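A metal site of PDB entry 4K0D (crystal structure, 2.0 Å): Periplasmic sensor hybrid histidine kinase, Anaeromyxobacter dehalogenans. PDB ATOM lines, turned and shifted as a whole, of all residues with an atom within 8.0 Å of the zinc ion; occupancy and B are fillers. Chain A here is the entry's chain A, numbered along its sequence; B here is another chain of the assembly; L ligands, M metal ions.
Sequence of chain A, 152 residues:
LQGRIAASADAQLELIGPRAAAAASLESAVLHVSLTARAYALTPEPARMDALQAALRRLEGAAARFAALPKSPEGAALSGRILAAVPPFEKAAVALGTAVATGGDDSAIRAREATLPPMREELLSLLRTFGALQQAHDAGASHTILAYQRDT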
ATOM      1  N   ALA A   6     -37.040  12.693  -5.223  1.00  0.00           N
ATOM      2  CA  ALA A   6     -35.825  12.745  -6.038  1.00  0.00           C
ATOM      3  C   ALA A   6     -34.884  11.706  -5.424  1.00  0.00           C
ATOM      4  O   ALA A   6     -34.212  10.953  -6.133  1.00  0.00           O
ATOM      5  CB  ALA A   6     -35.210  14.139  -5.976  1.00  0.00           C
ATOM      6  N   ALA A   7     -34.843  11.698  -4.101  1.00  0.00           N
ATOM      7  CA  ALA A   7     -34.057  10.712  -3.391  1.00  0.00           C
ATOM      8  C   ALA A   7     -34.546   9.276  -3.674  1.00  0.00           C
ATOM      9  O   ALA A   7     -33.737   8.375  -3.800  1.00  0.00           O
ATOM     10  CB  ALA A   7     -34.057  11.001  -1.882  1.00  0.00           C
ATOM     11  N   ALA A   9     -36.304   8.335  -6.415  1.00  0.00           N
ATOM     12  CA  ALA A   9     -35.960   8.035  -7.816  1.00  0.00           C
ATOM     13  C   ALA A   9     -34.515   7.529  -7.842  1.00  0.00           C
ATOM     14  O   ALA A   9     -34.239   6.458  -8.360  1.00  0.00           O
ATOM     15  CB  ALA A   9     -36.083   9.241  -8.694  1.00  0.00           C
ATOM     16  N   ASP A  10     -33.611   8.306  -7.239  1.00  0.00           N
ATOM     17  CA  ASP A  10     -32.210   8.030  -7.363  1.00  0.00           C
ATOM     18  C   ASP A  10     -31.922   6.692  -6.767  1.00  0.00           C
ATOM     19  O   ASP A  10     -31.202   5.940  -7.316  1.00  0.00           O
ATOM     20  CB  ASP A  10     -31.330   9.059  -6.703  1.00  0.00           C
ATOM     21  CG  ASP A  10     -29.884   8.853  -7.098  1.00  0.00           C
ATOM     22  OD1 ASP A  10     -29.705   8.325  -8.197  1.00  0.00           O
ATOM     23  OD2 ASP A  10     -28.932   9.177  -6.349  1.00  0.00           O
ATOM     24  N   ALA A  11     -32.530   6.391  -5.638  1.00  0.00           N
ATOM     25  CA  ALA A  11     -32.445   5.067  -5.064  1.00  0.00           C
ATOM     26  C   ALA A  11     -32.853   3.982  -6.100  1.00  0.00           C
ATOM     27  O   ALA A  11     -32.243   2.921  -6.167  1.00  0.00           O
ATOM     28  CB  ALA A  11     -33.349   4.999  -3.872  1.00  0.00           C
ATOM     29  N   GLN A  12     -33.885   4.237  -6.891  1.00  0.00           N
ATOM     30  CA  GLN A  12     -34.288   3.235  -7.881  1.00  0.00           C
ATOM     31  C   GLN A  12     -33.192   3.019  -8.878  1.00  0.00           C
ATOM     32  O   GLN A  12     -32.823   1.854  -9.227  1.00  0.00           O
ATOM     33  CB  GLN A  12     -35.542   3.689  -8.637  1.00  0.00           C
ATOM     34  CG  GLN A  12     -36.841   3.456  -7.919  1.00  0.00           C
ATOM     35  N   LEU A  13     -32.660   4.128  -9.388  1.00  0.00           N
ATOM     36  CA  LEU A  13     -31.741   3.999 -10.521  1.00  0.00           C
ATOM     37  C   LEU A  13     -30.429   3.395 -10.105  1.00  0.00           C
ATOM     38  O   LEU A  13     -29.708   2.792 -10.915  1.00  0.00           O
ATOM     39  CB  LEU A  13     -31.480   5.348 -11.184  1.00  0.00           C
ATOM     40  CG  LEU A  13     -32.746   5.914 -11.746  1.00  0.00           C
ATOM     41  CD1 LEU A  13     -32.378   7.163 -12.514  1.00  0.00           C
ATOM     42  CD2 LEU A  13     -33.438   4.873 -12.659  1.00  0.00           C
ATOM     43  N   GLU A  14     -30.110   3.553  -8.837  1.00  0.00           N
ATOM     44  CA  GLU A  14     -28.821   3.116  -8.310  1.00  0.00           C
ATOM     45  C   GLU A  14     -28.765   1.621  -8.082  1.00  0.00           C
ATOM     46  O   GLU A  14     -27.716   1.059  -7.767  1.00  0.00           O
ATOM     47  CB  GLU A  14     -28.590   3.859  -7.001  1.00  0.00           C
ATOM     48  CG  GLU A  14     -28.328   5.350  -7.232  1.00  0.00           C
ATOM     49  CD  GLU A  14     -26.989   5.571  -7.916  1.00  0.00           C
ATOM     50  OE1 GLU A  14     -26.167   4.610  -8.129  1.00  0.00           O
ATOM     51  OE2 GLU A  14     -26.750   6.731  -8.219  1.00  0.00           O
ATOM     52  N   LEU A  15     -29.914   0.970  -8.171  1.00  0.00           N
ATOM     53  CA  LEU A  15     -29.913  -0.465  -8.206  1.00  0.00           C
ATOM     54  C   LEU A  15     -29.256  -1.055  -9.486  1.00  0.00           C
ATOM     55  O   LEU A  15     -28.748  -2.173  -9.467  1.00  0.00           O
ATOM     56  CB  LEU A  15     -31.348  -0.934  -8.122  1.00  0.00           C
ATOM     57  CG  LEU A  15     -31.930  -0.619  -6.766  1.00  0.00           C
ATOM     58  CD1 LEU A  15     -33.372  -1.016  -6.665  1.00  0.00           C
ATOM     59  CD2 LEU A  15     -31.137  -1.368  -5.737  1.00  0.00           C
ATOM     60  N   SER B  28     -24.067   3.432 -14.831  1.00  0.00           N
ATOM     61  CA  SER B  28     -24.661   4.105 -13.632  1.00  0.00           C
ATOM     62  C   SER B  28     -23.992   5.486 -13.274  1.00  0.00           C
ATOM     63  O   SER B  28     -24.703   6.502 -13.002  1.00  0.00           O
ATOM     64  CB  SER B  28     -24.609   3.128 -12.469  1.00  0.00           C
ATOM     65  OG  SER B  28     -25.552   3.404 -11.477  1.00  0.00           O
ATOM     66  N   ALA B  29     -22.685   5.587 -13.377  1.00  0.00           N
ATOM     67  CA  ALA B  29     -21.994   6.840 -13.020  1.00  0.00           C
ATOM     68  C   ALA B  29     -22.436   7.923 -14.023  1.00  0.00           C
ATOM     69  O   ALA B  29     -22.530   9.112 -13.730  1.00  0.00           O
ATOM     70  CB  ALA B  29     -20.440   6.633 -13.060  1.00  0.00           C
ATOM     71  N   VAL B  30     -22.671   7.516 -15.247  1.00  0.00           N
ATOM     72  CA  VAL B  30     -23.026   8.440 -16.268  1.00  0.00           C
ATOM     73  C   VAL B  30     -24.450   8.931 -16.000  1.00  0.00           C
ATOM     74  O   VAL B  30     -24.693  10.142 -16.008  1.00  0.00           O
ATOM     75  CB  VAL B  30     -22.896   7.822 -17.700  1.00  0.00           C
ATOM     76  CG1 VAL B  30     -23.598   8.656 -18.733  1.00  0.00           C
ATOM     77  CG2 VAL B  30     -21.467   7.695 -18.039  1.00  0.00           C
ATOM     78  N   LEU B  31     -25.367   7.998 -15.712  1.00  0.00           N
ATOM     79  CA  LEU B  31     -26.714   8.392 -15.331  1.00  0.00           C
ATOM     80  C   LEU B  31     -26.644   9.338 -14.165  1.00  0.00           C
ATOM     81  O   LEU B  31     -27.360  10.326 -14.124  1.00  0.00           O
ATOM     82  CB  LEU B  31     -27.550   7.210 -14.888  1.00  0.00           C
ATOM     83  CG  LEU B  31     -28.054   6.402 -16.084  1.00  0.00           C
ATOM     84  CD1 LEU B  31     -28.623   5.055 -15.705  1.00  0.00           C
ATOM     85  CD2 LEU B  31     -29.113   7.205 -16.830  1.00  0.00           C
ATOM     86  N   HIS B  32     -25.804   9.008 -13.196  1.00  0.00           N
ATOM     87  CA  HIS B  32     -25.816   9.689 -11.917  1.00  0.00           C
ATOM     88  C   HIS B  32     -25.310  11.122 -12.143  1.00  0.00           C
ATOM     89  O   HIS B  32     -25.829  12.053 -11.555  1.00  0.00           O
ATOM     90  CB  HIS B  32     -25.040   8.934 -10.821  1.00  0.00           C
ATOM     91  CG  HIS B  32     -25.162   9.576  -9.452  1.00  0.00           C
ATOM     92  ND1 HIS B  32     -26.255   9.417  -8.651  1.00  0.00           N
ATOM     93  CD2 HIS B  32     -24.318  10.394  -8.779  1.00  0.00           C
ATOM     94  CE1 HIS B  32     -26.124  10.132  -7.543  1.00  0.00           C
ATOM     95  NE2 HIS B  32     -24.947  10.734  -7.593  1.00  0.00           N
ATOM     96  N   VAL B  33     -24.336  11.310 -13.021  1.00  0.00           N
ATOM     97  CA  VAL B  33     -23.908  12.672 -13.307  1.00  0.00           C
ATOM     98  C   VAL B  33     -25.073  13.440 -13.969  1.00  0.00           C
ATOM     99  O   VAL B  33     -25.277  14.591 -13.710  1.00  0.00           O
ATOM    100  CB  VAL B  33     -22.678  12.731 -14.233  1.00  0.00           C
ATOM    101  CG1 VAL B  33     -22.551  14.112 -14.816  1.00  0.00           C
ATOM    102  CG2 VAL B  33     -21.306  12.300 -13.462  1.00  0.00           C
ATOM    103  N   SER B  34     -25.818  12.788 -14.865  1.00  0.00           N
ATOM    104  CA  SER B  34     -26.956  13.425 -15.472  1.00  0.00           C
ATOM    105  C   SER B  34     -28.007  13.762 -14.486  1.00  0.00           C
ATOM    106  O   SER B  34     -28.593  14.826 -14.583  1.00  0.00           O
ATOM    107  CB  SER B  34     -27.571  12.534 -16.550  1.00  0.00           C
ATOM    108  OG  SER B  34     -26.867  12.775 -17.737  1.00  0.00           O
ATOM    109  N   LEU B  35     -28.274  12.858 -13.554  1.00  0.00           N
ATOM    110  CA  LEU B  35     -29.352  13.093 -12.629  1.00  0.00           C
ATOM    111  C   LEU B  35     -29.016  14.201 -11.642  1.00  0.00           C
ATOM    112  O   LEU B  35     -29.877  15.006 -11.366  1.00  0.00           O
ATOM    113  CB  LEU B  35     -29.719  11.841 -11.891  1.00  0.00           C
ATOM    114  CG  LEU B  35     -30.699  11.979 -10.739  1.00  0.00           C
ATOM    115  CD1 LEU B  35     -31.517  10.717 -10.506  1.00  0.00           C
ATOM    116  CD2 LEU B  35     -29.889  12.239  -9.518  1.00  0.00           C
ATOM    117  N   THR B  36     -27.800  14.260 -11.138  1.00  0.00           N
ATOM    118  CA  THR B  36     -27.424  15.291 -10.174  1.00  0.00           C
ATOM    119  C   THR B  36     -27.277  16.622 -10.902  1.00  0.00           C
ATOM    120  O   THR B  36     -27.529  17.656 -10.337  1.00  0.00           O
ATOM    121  CB  THR B  36     -26.100  14.959  -9.426  1.00  0.00           C
ATOM    122  OG1 THR B  36     -25.050  14.670 -10.379  1.00  0.00           O
ATOM    123  CG2 THR B  36     -26.284  13.757  -8.525  1.00  0.00           C
ATOM    124  N   ALA B  55     -20.649  13.151  -7.964  1.00  0.00           N
ATOM    125  CA  ALA B  55     -20.979  12.280  -9.107  1.00  0.00           C
ATOM    126  C   ALA B  55     -19.858  12.325 -10.106  1.00  0.00           C
ATOM    127  O   ALA B  55     -19.571  11.355 -10.744  1.00  0.00           O
ATOM    128  CB  ALA B  55     -22.328  12.722  -9.799  1.00  0.00           C
ATOM    129  N   ARG B  58     -17.049  10.063  -8.867  1.00  0.00           N
ATOM    130  CA  ARG B  58     -17.503   8.729  -9.112  1.00  0.00           C
ATOM    131  C   ARG B  58     -17.378   8.304 -10.612  1.00  0.00           C
ATOM    132  O   ARG B  58     -16.934   7.212 -10.914  1.00  0.00           O
ATOM    133  CB  ARG B  58     -18.916   8.605  -8.652  1.00  0.00           C
ATOM    134  CG  ARG B  58     -19.510   7.308  -8.999  1.00  0.00           C
ATOM    135  CD  ARG B  58     -20.899   7.241  -8.413  1.00  0.00           C
ATOM    136  NE  ARG B  58     -21.677   6.154  -8.970  1.00  0.00           N
ATOM    137  CZ  ARG B  58     -22.978   6.005  -8.813  1.00  0.00           C
ATOM    138  NH1 ARG B  58     -23.667   6.851  -8.052  1.00  0.00           N
ATOM    139  NH2 ARG B  58     -23.610   5.000  -9.421  1.00  0.00           N
HETATM  140 CL1  LIG L   1     -28.553   7.712 -11.102  1.00  0.00          CL
HETATM  141 ZN    ZN M   1     -27.820   8.152  -8.974  1.00  0.00          ZN
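Three residues have an atom within 4 Å of the zinc ion: Asp 10, Glu 14 and His 32 of chain B.
The nearest printed residue that does not touch the zinc ion is Arg 58 of chain B (4.4 Å).
The side-chain carboxylate (OE2) of Glu 14 is bound to the zinc ion, at 1.9 Å.
ND1 of His 32 of chain B is bound to the zinc ion, 2.0 Å away.
The zinc ion is bound by OD1 of Asp 10 (2.0 Å).
CL1 of the ligand binds the zinc ion, at 2.3 Å.
The zinc ion has four donor atoms within binding distance.
The side-chain carboxylate (OE1) of Glu 14 is in salt-bridge range of the guanidinium group (NH2) of Arg 58 of chain B.
The backbone carbonyl oxygen of His 32 of chain B lies within hydrogen-bond range of the side-chain hydroxyl of Thr 36 of chain B.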
